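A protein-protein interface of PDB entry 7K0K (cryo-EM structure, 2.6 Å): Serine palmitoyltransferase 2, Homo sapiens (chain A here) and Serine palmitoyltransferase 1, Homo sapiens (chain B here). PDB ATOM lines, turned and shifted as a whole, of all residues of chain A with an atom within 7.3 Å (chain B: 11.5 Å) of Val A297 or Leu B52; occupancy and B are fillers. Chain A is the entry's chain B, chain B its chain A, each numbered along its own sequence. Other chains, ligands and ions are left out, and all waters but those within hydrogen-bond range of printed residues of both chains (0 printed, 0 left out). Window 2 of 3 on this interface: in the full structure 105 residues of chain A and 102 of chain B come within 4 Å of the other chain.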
ATOM      1  N   LEU A 291      -9.007 -35.480   5.722  1.00  0.00           N
ATOM      2  CA  LEU A 291      -7.954 -35.294   4.731  1.00  0.00           C
ATOM      3  C   LEU A 291      -7.578 -33.829   4.593  1.00  0.00           C
ATOM      4  O   LEU A 291      -6.395 -33.496   4.487  1.00  0.00           O
ATOM      5  CB  LEU A 291      -8.382 -35.859   3.381  1.00  0.00           C
ATOM      6  CG  LEU A 291      -8.344 -37.374   3.222  1.00  0.00           C
ATOM      7  CD1 LEU A 291      -8.627 -37.729   1.789  1.00  0.00           C
ATOM      8  CD2 LEU A 291      -6.998 -37.911   3.644  1.00  0.00           C
ATOM      9  N   LEU A 292      -8.567 -32.937   4.589  1.00  0.00           N
ATOM     10  CA  LEU A 292      -8.282 -31.510   4.486  1.00  0.00           C
ATOM     11  C   LEU A 292      -7.478 -31.025   5.685  1.00  0.00           C
ATOM     12  O   LEU A 292      -6.486 -30.299   5.533  1.00  0.00           O
ATOM     13  CB  LEU A 292      -9.589 -30.730   4.365  1.00  0.00           C
ATOM     14  CG  LEU A 292     -10.147 -30.552   2.956  1.00  0.00           C
ATOM     15  CD1 LEU A 292     -11.624 -30.232   3.012  1.00  0.00           C
ATOM     16  CD2 LEU A 292      -9.389 -29.470   2.221  1.00  0.00           C
ATOM     17  N   LYS A 293      -7.890 -31.427   6.890  1.00  0.00           N
ATOM     18  CA  LYS A 293      -7.165 -31.048   8.096  1.00  0.00           C
ATOM     19  C   LYS A 293      -5.715 -31.491   8.021  1.00  0.00           C
ATOM     20  O   LYS A 293      -4.797 -30.686   8.219  1.00  0.00           O
ATOM     21  CB  LYS A 293      -7.831 -31.665   9.325  1.00  0.00           C
ATOM     22  CG  LYS A 293      -8.967 -30.869   9.916  1.00  0.00           C
ATOM     23  CD  LYS A 293      -9.637 -31.660  11.026  1.00  0.00           C
ATOM     24  CE  LYS A 293     -10.455 -30.764  11.937  1.00  0.00           C
ATOM     25  NZ  LYS A 293      -9.626 -29.686  12.532  1.00  0.00           N
ATOM     26  N   ASP A 294      -5.492 -32.774   7.732  1.00  0.00           N
ATOM     27  CA  ASP A 294      -4.133 -33.299   7.706  1.00  0.00           C
ATOM     28  C   ASP A 294      -3.305 -32.645   6.611  1.00  0.00           C
ATOM     29  O   ASP A 294      -2.126 -32.342   6.814  1.00  0.00           O
ATOM     30  CB  ASP A 294      -4.162 -34.811   7.523  1.00  0.00           C
ATOM     31  CG  ASP A 294      -4.790 -35.520   8.695  1.00  0.00           C
ATOM     32  OD1 ASP A 294      -5.400 -34.835   9.540  1.00  0.00           O
ATOM     33  OD2 ASP A 294      -4.674 -36.760   8.772  1.00  0.00           O
ATOM     34  N   ALA A 295      -3.902 -32.424   5.441  1.00  0.00           N
ATOM     35  CA  ALA A 295      -3.172 -31.819   4.338  1.00  0.00           C
ATOM     36  C   ALA A 295      -2.717 -30.413   4.687  1.00  0.00           C
ATOM     37  O   ALA A 295      -1.575 -30.033   4.415  1.00  0.00           O
ATOM     38  CB  ALA A 295      -4.046 -31.802   3.090  1.00  0.00           C
ATOM     39  N   ILE A 296      -3.600 -29.618   5.291  1.00  0.00           N
ATOM     40  CA  ILE A 296      -3.214 -28.256   5.639  1.00  0.00           C
ATOM     41  C   ILE A 296      -2.179 -28.264   6.755  1.00  0.00           C
ATOM     42  O   ILE A 296      -1.211 -27.495   6.725  1.00  0.00           O
ATOM     43  CB  ILE A 296      -4.449 -27.423   6.016  1.00  0.00           C
ATOM     44  CG1 ILE A 296      -5.382 -27.291   4.817  1.00  0.00           C
ATOM     45  CG2 ILE A 296      -4.035 -26.051   6.494  1.00  0.00           C
ATOM     46  CD1 ILE A 296      -6.698 -26.657   5.152  1.00  0.00           C
ATOM     47  N   VAL A 297      -2.355 -29.132   7.752  1.00  0.00           N
ATOM     48  CA  VAL A 297      -1.478 -29.091   8.917  1.00  0.00           C
ATOM     49  C   VAL A 297      -0.077 -29.579   8.570  1.00  0.00           C
ATOM     50  O   VAL A 297       0.918 -28.944   8.935  1.00  0.00           O
ATOM     51  CB  VAL A 297      -2.088 -29.900  10.072  1.00  0.00           C
ATOM     52  CG1 VAL A 297      -1.065 -30.109  11.163  1.00  0.00           C
ATOM     53  CG2 VAL A 297      -3.299 -29.182  10.623  1.00  0.00           C
ATOM     54  N   TYR A 298       0.031 -30.699   7.858  1.00  0.00           N
ATOM     55  CA  TYR A 298       1.316 -31.367   7.699  1.00  0.00           C
ATOM     56  C   TYR A 298       2.035 -31.036   6.401  1.00  0.00           C
ATOM     57  O   TYR A 298       3.192 -31.432   6.242  1.00  0.00           O
ATOM     58  CB  TYR A 298       1.130 -32.882   7.803  1.00  0.00           C
ATOM     59  CG  TYR A 298       0.585 -33.304   9.148  1.00  0.00           C
ATOM     60  CD1 TYR A 298       1.314 -33.095  10.306  1.00  0.00           C
ATOM     61  CD2 TYR A 298      -0.667 -33.883   9.259  1.00  0.00           C
ATOM     62  CE1 TYR A 298       0.822 -33.467  11.532  1.00  0.00           C
ATOM     63  CE2 TYR A 298      -1.169 -34.255  10.481  1.00  0.00           C
ATOM     64  CZ  TYR A 298      -0.421 -34.045  11.615  1.00  0.00           C
ATOM     65  OH  TYR A 298      -0.918 -34.417  12.840  1.00  0.00           O
ATOM     66  N   GLY A 299       1.396 -30.335   5.477  1.00  0.00           N
ATOM     67  CA  GLY A 299       2.089 -29.881   4.291  1.00  0.00           C
ATOM     68  C   GLY A 299       2.451 -31.005   3.337  1.00  0.00           C
ATOM     69  O   GLY A 299       1.953 -32.128   3.420  1.00  0.00           O
ATOM     70  N   GLN A 300       3.351 -30.679   2.413  1.00  0.00           N
ATOM     71  CA  GLN A 300       3.754 -31.625   1.387  1.00  0.00           C
ATOM     72  C   GLN A 300       4.569 -32.764   2.001  1.00  0.00           C
ATOM     73  O   GLN A 300       5.272 -32.569   2.994  1.00  0.00           O
ATOM     74  CB  GLN A 300       4.550 -30.911   0.301  1.00  0.00           C
ATOM     75  CG  GLN A 300       3.864 -29.657  -0.199  1.00  0.00           C
ATOM     76  CD  GLN A 300       4.559 -29.047  -1.384  1.00  0.00           C
ATOM     77  OE1 GLN A 300       5.326 -29.710  -2.075  1.00  0.00           O
ATOM     78  NE2 GLN A 300       4.297 -27.772  -1.629  1.00  0.00           N
ATOM     79  N   ARG A 304       7.925 -30.763   4.433  1.00  0.00           N
ATOM     80  CA  ARG A 304       6.642 -30.401   5.028  1.00  0.00           C
ATOM     81  C   ARG A 304       6.337 -28.918   4.809  1.00  0.00           C
ATOM     82  O   ARG A 304       6.018 -28.164   5.726  1.00  0.00           O
ATOM     83  CB  ARG A 304       6.639 -30.769   6.504  1.00  0.00           C
ATOM     84  CG  ARG A 304       6.690 -32.263   6.751  1.00  0.00           C
ATOM     85  CD  ARG A 304       6.713 -32.564   8.231  1.00  0.00           C
ATOM     86  NE  ARG A 304       5.473 -32.179   8.888  1.00  0.00           N
ATOM     87  CZ  ARG A 304       5.300 -32.188  10.204  1.00  0.00           C
ATOM     88  NH1 ARG A 304       4.142 -31.812  10.727  1.00  0.00           N
ATOM     89  NH2 ARG A 304       6.286 -32.576  11.000  1.00  0.00           N
ATOM     90  N   ARG A 305       6.410 -28.520   3.541  1.00  0.00           N
ATOM     91  CA  ARG A 305       6.050 -27.190   3.089  1.00  0.00           C
ATOM     92  C   ARG A 305       4.539 -27.094   2.903  1.00  0.00           C
ATOM     93  O   ARG A 305       3.892 -28.075   2.536  1.00  0.00           O
ATOM     94  CB  ARG A 305       6.741 -26.870   1.771  1.00  0.00           C
ATOM     95  CG  ARG A 305       8.192 -26.474   1.891  1.00  0.00           C
ATOM     96  CD  ARG A 305       8.342 -25.129   2.563  1.00  0.00           C
ATOM     97  NE  ARG A 305       9.725 -24.666   2.560  1.00  0.00           N
ATOM     98  CZ  ARG A 305      10.623 -24.991   3.481  1.00  0.00           C
ATOM     99  NH1 ARG A 305      11.857 -24.520   3.397  1.00  0.00           N
ATOM    100  NH2 ARG A 305      10.292 -25.793   4.481  1.00  0.00           N
ATOM    101  N   PRO A 306       3.955 -25.924   3.146  1.00  0.00           N
ATOM    102  CA  PRO A 306       2.524 -25.754   2.879  1.00  0.00           C
ATOM    103  C   PRO A 306       2.205 -25.956   1.406  1.00  0.00           C
ATOM    104  O   PRO A 306       2.989 -25.595   0.526  1.00  0.00           O
ATOM    105  CB  PRO A 306       2.253 -24.313   3.324  1.00  0.00           C
ATOM    106  CG  PRO A 306       3.592 -23.662   3.357  1.00  0.00           C
ATOM    107  CD  PRO A 306       4.541 -24.727   3.764  1.00  0.00           C
ATOM    108  N   TRP A 307       1.041 -26.542   1.141  1.00  0.00           N
ATOM    109  CA  TRP A 307       0.610 -26.774  -0.231  1.00  0.00           C
ATOM    110  C   TRP A 307       0.335 -25.453  -0.932  1.00  0.00           C
ATOM    111  O   TRP A 307      -0.086 -24.476  -0.308  1.00  0.00           O
ATOM    112  CB  TRP A 307      -0.654 -27.630  -0.262  1.00  0.00           C
ATOM    113  CG  TRP A 307      -0.511 -29.006   0.293  1.00  0.00           C
ATOM    114  CD1 TRP A 307      -0.859 -29.416   1.539  1.00  0.00           C
ATOM    115  CD2 TRP A 307      -0.022 -30.164  -0.387  1.00  0.00           C
ATOM    116  NE1 TRP A 307      -0.604 -30.752   1.687  1.00  0.00           N
ATOM    117  CE2 TRP A 307      -0.086 -31.236   0.517  1.00  0.00           C
ATOM    118  CE3 TRP A 307       0.479 -30.397  -1.669  1.00  0.00           C
ATOM    119  CZ2 TRP A 307       0.324 -32.516   0.182  1.00  0.00           C
ATOM    120  CZ3 TRP A 307       0.886 -31.668  -1.997  1.00  0.00           C
ATOM    121  CH2 TRP A 307       0.808 -32.712  -1.077  1.00  0.00           C
ATOM    122  N   ILE A 310      -5.250 -26.627  -2.860  1.00  0.00           N
ATOM    123  CA  ILE A 310      -5.952 -27.878  -2.595  1.00  0.00           C
ATOM    124  C   ILE A 310      -7.204 -27.884  -3.455  1.00  0.00           C
ATOM    125  O   ILE A 310      -8.060 -27.005  -3.313  1.00  0.00           O
ATOM    126  CB  ILE A 310      -6.305 -28.055  -1.113  1.00  0.00           C
ATOM    127  CG1 ILE A 310      -5.033 -28.193  -0.278  1.00  0.00           C
ATOM    128  CG2 ILE A 310      -7.187 -29.267  -0.930  1.00  0.00           C
ATOM    129  CD1 ILE A 310      -5.289 -28.509   1.172  1.00  0.00           C
ATOM    130  N   ASP B  51       1.910 -35.479  19.339  1.00  0.00           N
ATOM    131  CA  ASP B  51       2.626 -34.499  18.535  1.00  0.00           C
ATOM    132  C   ASP B  51       2.088 -33.094  18.784  1.00  0.00           C
ATOM    133  O   ASP B  51       2.154 -32.588  19.903  1.00  0.00           O
ATOM    134  CB  ASP B  51       2.530 -34.852  17.051  1.00  0.00           C
ATOM    135  N   LEU B  52       1.555 -32.469  17.736  1.00  0.00           N
ATOM    136  CA  LEU B  52       1.098 -31.090  17.835  1.00  0.00           C
ATOM    137  C   LEU B  52      -0.145 -30.986  18.705  1.00  0.00           C
ATOM    138  O   LEU B  52      -0.947 -31.920  18.791  1.00  0.00           O
ATOM    139  CB  LEU B  52       0.793 -30.527  16.449  1.00  0.00           C
ATOM    140  CG  LEU B  52       1.925 -30.396  15.435  1.00  0.00           C
ATOM    141  CD1 LEU B  52       1.351 -30.065  14.073  1.00  0.00           C
ATOM    142  CD2 LEU B  52       2.919 -29.333  15.864  1.00  0.00           C
ATOM    143  N   THR B  53      -0.302 -29.836  19.352  1.00  0.00           N
ATOM    144  CA  THR B  53      -1.519 -29.535  20.084  1.00  0.00           C
ATOM    145  C   THR B  53      -2.647 -29.222  19.110  1.00  0.00           C
ATOM    146  O   THR B  53      -2.421 -28.850  17.959  1.00  0.00           O
ATOM    147  CB  THR B  53      -1.291 -28.359  21.033  1.00  0.00           C
ATOM    148  OG1 THR B  53      -0.026 -28.516  21.683  1.00  0.00           O
ATOM    149  CG2 THR B  53      -2.375 -28.290  22.093  1.00  0.00           C
ATOM    150  N   VAL B  54      -3.881 -29.403  19.581  1.00  0.00           N
ATOM    151  CA  VAL B  54      -5.049 -29.059  18.775  1.00  0.00           C
ATOM    152  C   VAL B  54      -5.113 -27.555  18.541  1.00  0.00           C
ATOM    153  O   VAL B  54      -5.536 -27.095  17.472  1.00  0.00           O
ATOM    154  CB  VAL B  54      -6.330 -29.603  19.435  1.00  0.00           C
ATOM    155  CG1 VAL B  54      -6.579 -28.930  20.770  1.00  0.00           C
ATOM    156  CG2 VAL B  54      -7.521 -29.414  18.515  1.00  0.00           C
ATOM    157  N   LYS B  55      -4.687 -26.764  19.527  1.00  0.00           N
ATOM    158  CA  LYS B  55      -4.645 -25.317  19.350  1.00  0.00           C
ATOM    159  C   LYS B  55      -3.634 -24.921  18.280  1.00  0.00           C
ATOM    160  O   LYS B  55      -3.916 -24.063  17.436  1.00  0.00           O
ATOM    161  CB  LYS B  55      -4.324 -24.641  20.682  1.00  0.00           C
ATOM    162  CG  LYS B  55      -4.112 -23.141  20.590  1.00  0.00           C
ATOM    163  CD  LYS B  55      -3.757 -22.559  21.946  1.00  0.00           C
ATOM    164  CE  LYS B  55      -3.388 -21.090  21.841  1.00  0.00           C
ATOM    165  NZ  LYS B  55      -4.430 -20.313  21.115  1.00  0.00           N
ATOM    166  N   GLU B  56      -2.458 -25.545  18.287  1.00  0.00           N
ATOM    167  CA  GLU B  56      -1.478 -25.281  17.241  1.00  0.00           C
ATOM    168  C   GLU B  56      -2.020 -25.665  15.872  1.00  0.00           C
ATOM    169  O   GLU B  56      -1.802 -24.953  14.886  1.00  0.00           O
ATOM    170  CB  GLU B  56      -0.185 -26.043  17.525  1.00  0.00           C
ATOM    171  CG  GLU B  56       0.469 -25.686  18.839  1.00  0.00           C
ATOM    172  CD  GLU B  56       1.486 -26.716  19.270  1.00  0.00           C
ATOM    173  OE1 GLU B  56       2.077 -27.369  18.388  1.00  0.00           O
ATOM    174  OE2 GLU B  56       1.693 -26.877  20.490  1.00  0.00           O
ATOM    175  N   LYS B  57      -2.713 -26.799  15.789  1.00  0.00           N
ATOM    176  CA  LYS B  57      -3.235 -27.250  14.506  1.00  0.00           C
ATOM    177  C   LYS B  57      -4.303 -26.304  13.983  1.00  0.00           C
ATOM    178  O   LYS B  57      -4.339 -25.999  12.785  1.00  0.00           O
ATOM    179  CB  LYS B  57      -3.775 -28.673  14.635  1.00  0.00           C
ATOM    180  CG  LYS B  57      -2.684 -29.714  14.797  1.00  0.00           C
ATOM    181  CD  LYS B  57      -3.219 -31.126  14.695  1.00  0.00           C
ATOM    182  CE  LYS B  57      -4.105 -31.468  15.874  1.00  0.00           C
ATOM    183  NZ  LYS B  57      -4.489 -32.903  15.880  1.00  0.00           N
ATOM    184  N   GLU B  58      -5.177 -25.815  14.864  1.00  0.00           N
ATOM    185  CA  GLU B  58      -6.195 -24.877  14.412  1.00  0.00           C
ATOM    186  C   GLU B  58      -5.573 -23.540  14.028  1.00  0.00           C
ATOM    187  O   GLU B  58      -6.039 -22.880  13.091  1.00  0.00           O
ATOM    188  CB  GLU B  58      -7.281 -24.705  15.474  1.00  0.00           C
ATOM    189  CG  GLU B  58      -6.896 -23.899  16.691  1.00  0.00           C
ATOM    190  CD  GLU B  58      -7.727 -24.260  17.902  1.00  0.00           C
ATOM    191  OE1 GLU B  58      -7.419 -23.768  19.007  1.00  0.00           O
ATOM    192  OE2 GLU B  58      -8.692 -25.036  17.747  1.00  0.00           O
ATOM    193  N   GLU B  59      -4.500 -23.135  14.713  1.00  0.00           N
ATOM    194  CA  GLU B  59      -3.775 -21.939  14.292  1.00  0.00           C
ATOM    195  C   GLU B  59      -3.177 -22.118  12.903  1.00  0.00           C
ATOM    196  O   GLU B  59      -3.239 -21.208  12.069  1.00  0.00           O
ATOM    197  CB  GLU B  59      -2.677 -21.607  15.297  1.00  0.00           C
ATOM    198  CG  GLU B  59      -3.181 -21.098  16.626  1.00  0.00           C
ATOM    199  CD  GLU B  59      -2.102 -21.088  17.687  1.00  0.00           C
ATOM    200  OE1 GLU B  59      -0.953 -21.463  17.376  1.00  0.00           O
ATOM    201  OE2 GLU B  59      -2.405 -20.709  18.836  1.00  0.00           O
ATOM    202  N   LEU B  60      -2.584 -23.284  12.644  1.00  0.00           N
ATOM    203  CA  LEU B  60      -2.010 -23.561  11.332  1.00  0.00           C
ATOM    204  C   LEU B  60      -3.073 -23.530  10.250  1.00  0.00           C
ATOM    205  O   LEU B  60      -2.841 -23.007   9.157  1.00  0.00           O
ATOM    206  CB  LEU B  60      -1.318 -24.923  11.340  1.00  0.00           C
ATOM    207  CG  LEU B  60       0.029 -25.054  12.034  1.00  0.00           C
ATOM    208  CD1 LEU B  60       0.339 -26.514  12.236  1.00  0.00           C
ATOM    209  CD2 LEU B  60       1.103 -24.396  11.209  1.00  0.00           C
ATOM    210  N   ILE B  61      -4.240 -24.112  10.529  1.00  0.00           N
ATOM    211  CA  ILE B  61      -5.334 -24.090   9.561  1.00  0.00           C
ATOM    212  C   ILE B  61      -5.787 -22.659   9.304  1.00  0.00           C
ATOM    213  O   ILE B  61      -6.044 -22.265   8.162  1.00  0.00           O
ATOM    214  CB  ILE B  61      -6.498 -24.972  10.046  1.00  0.00           C
ATOM    215  CG1 ILE B  61      -6.078 -26.438  10.075  1.00  0.00           C
ATOM    216  CG2 ILE B  61      -7.705 -24.794   9.155  1.00  0.00           C
ATOM    217  CD1 ILE B  61      -7.059 -27.332  10.790  1.00  0.00           C
ATOM    218  N   GLU B  62      -5.893 -21.859  10.366  1.00  0.00           N
ATOM    219  CA  GLU B  62      -6.331 -20.477  10.216  1.00  0.00           C
ATOM    220  C   GLU B  62      -5.344 -19.647   9.409  1.00  0.00           C
ATOM    221  O   GLU B  62      -5.760 -18.789   8.624  1.00  0.00           O
ATOM    222  CB  GLU B  62      -6.548 -19.849  11.592  1.00  0.00           C
ATOM    223  CG  GLU B  62      -6.936 -18.382  11.556  1.00  0.00           C
ATOM    224  CD  GLU B  62      -5.781 -17.457  11.903  1.00  0.00           C
ATOM    225  OE1 GLU B  62      -5.618 -16.423  11.223  1.00  0.00           O
ATOM    226  OE2 GLU B  62      -5.037 -17.761  12.861  1.00  0.00           O
ATOM    227  N   GLU B  63      -4.044 -19.876   9.579  1.00  0.00           N
ATOM    228  CA  GLU B  63      -3.054 -19.005   8.960  1.00  0.00           C
ATOM    229  C   GLU B  63      -2.657 -19.435   7.555  1.00  0.00           C
ATOM    230  O   GLU B  63      -1.831 -18.758   6.936  1.00  0.00           O
ATOM    231  CB  GLU B  63      -1.804 -18.920   9.838  1.00  0.00           C
ATOM    232  CG  GLU B  63      -1.037 -20.220   9.973  1.00  0.00           C
ATOM    233  CD  GLU B  63       0.156 -20.103  10.907  1.00  0.00           C
ATOM    234  OE1 GLU B  63       0.370 -19.008  11.468  1.00  0.00           O
ATOM    235  OE2 GLU B  63       0.887 -21.102  11.072  1.00  0.00           O
ATOM    236  N   TRP B  64      -3.208 -20.526   7.032  1.00  0.00           N
ATOM    237  CA  TRP B  64      -2.843 -21.025   5.713  1.00  0.00           C
ATOM    238  C   TRP B  64      -3.644 -20.299   4.644  1.00  0.00           C
ATOM    239  O   TRP B  64      -4.877 -20.299   4.679  1.00  0.00           O
ATOM    240  CB  TRP B  64      -3.080 -22.530   5.603  1.00  0.00           C
ATOM    241  CG  TRP B  64      -2.774 -23.078   4.241  1.00  0.00           C
ATOM    242  CD1 TRP B  64      -1.548 -23.188   3.660  1.00  0.00           C
ATOM    243  CD2 TRP B  64      -3.712 -23.596   3.292  1.00  0.00           C
ATOM    244  NE1 TRP B  64      -1.662 -23.737   2.410  1.00  0.00           N
ATOM    245  CE2 TRP B  64      -2.982 -23.998   2.161  1.00  0.00           C
ATOM    246  CE3 TRP B  64      -5.097 -23.760   3.291  1.00  0.00           C
ATOM    247  CZ2 TRP B  64      -3.589 -24.551   1.043  1.00  0.00           C
ATOM    248  CZ3 TRP B  64      -5.695 -24.306   2.183  1.00  0.00           C
ATOM    249  CH2 TRP B  64      -4.944 -24.696   1.074  1.00  0.00           C
ATOM    250  N   GLN B  65      -2.941 -19.687   3.696  1.00  0.00           N
ATOM    251  CA  GLN B  65      -3.570 -18.980   2.589  1.00  0.00           C
ATOM    252  C   GLN B  65      -3.159 -19.627   1.276  1.00  0.00           C
ATOM    253  O   GLN B  65      -1.970 -19.585   0.917  1.00  0.00           O
ATOM    254  CB  GLN B  65      -3.192 -17.500   2.595  1.00  0.00           C
ATOM    255  CG  GLN B  65      -3.836 -16.711   3.721  1.00  0.00           C
ATOM    256  CD  GLN B  65      -5.343 -16.857   3.744  1.00  0.00           C
ATOM    257  OE1 GLN B  65      -5.991 -16.898   2.700  1.00  0.00           O
ATOM    258  NE2 GLN B  65      -5.909 -16.931   4.939  1.00  0.00           N
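Of the printed residues of chain B, Val A297 touches Leu B52, Lys B57 and Ile B61. Printed residues of chain A within 4 Å of Leu B52: Val A297 (3.8 Å). Lys A293 touches just one residue of chain B: Ile B61. Ala A295 touches none of the printed residues of chain B. Printed residues of chain B within 4 Å of Ile A296: Ile B61 (3.9 Å) and Trp B64 (3.8 Å). Tyr A298 touches none of the printed residues of chain B. No residue of chain B comes within 4 Å of Gly A299. Printed residues of chain B within 4 Å of Ile A310: Trp B64 (3.8 Å). Printed residues of chain B within 4 Å of Trp A307: Trp B64 (3.2 Å). Of the printed residues of chain A, Lys B57 touches Val A297 (3.99 Å). The nearest printed residue of chain B that does not touch Val A297 is Leu B60 (4.01 Å).
NE1 of Trp A307 sits at hydrogen-bond distance from O of Ala A295. The backbone carbonyl oxygen (O) of Gly A299 lies within hydrogen-bond range of the indole nitrogen (NE1) of Trp A307, 3.4 Å away. The side-chain amide nitrogen (NE2) of Gln A300 lies within hydrogen-bond range of the backbone carbonyl oxygen (O) of Pro A306, at 3.3 Å.
NE1 of Trp B64 is in hydrogen-bond range of O of Trp A307, 3.2 Å away.
Hydrophobic or aromatic side chains of chain B within 4 Å of the printed part of chain A: Leu B52, Ile B61 and Trp B64. Of the 15 printed residues of chain A, 6 touch a printed residue of chain B. Hydrophobic or aromatic side chains of chain A within 4 Å of the printed part of chain B: Ile A296, Val A297, Pro A306 and Ile A310. Among the printed residues, 9 pairs touch across the chains.
Ile B61 touches Lys A293. Ile B61 touches Ile A296 (CA to CG2, 3.9 Å). Trp B64 touches Ile A296 (CB to CG2, 3.8 Å). Leu B52 touches Val A297. CG2 of Val A297 touches O of Lys B57 (3.99 Å). CG2 of Val A297 touches CG1 of Ile B61, at 3.9 Å. Pro A306 touches Trp B64. Ile A310 touches Trp B64.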
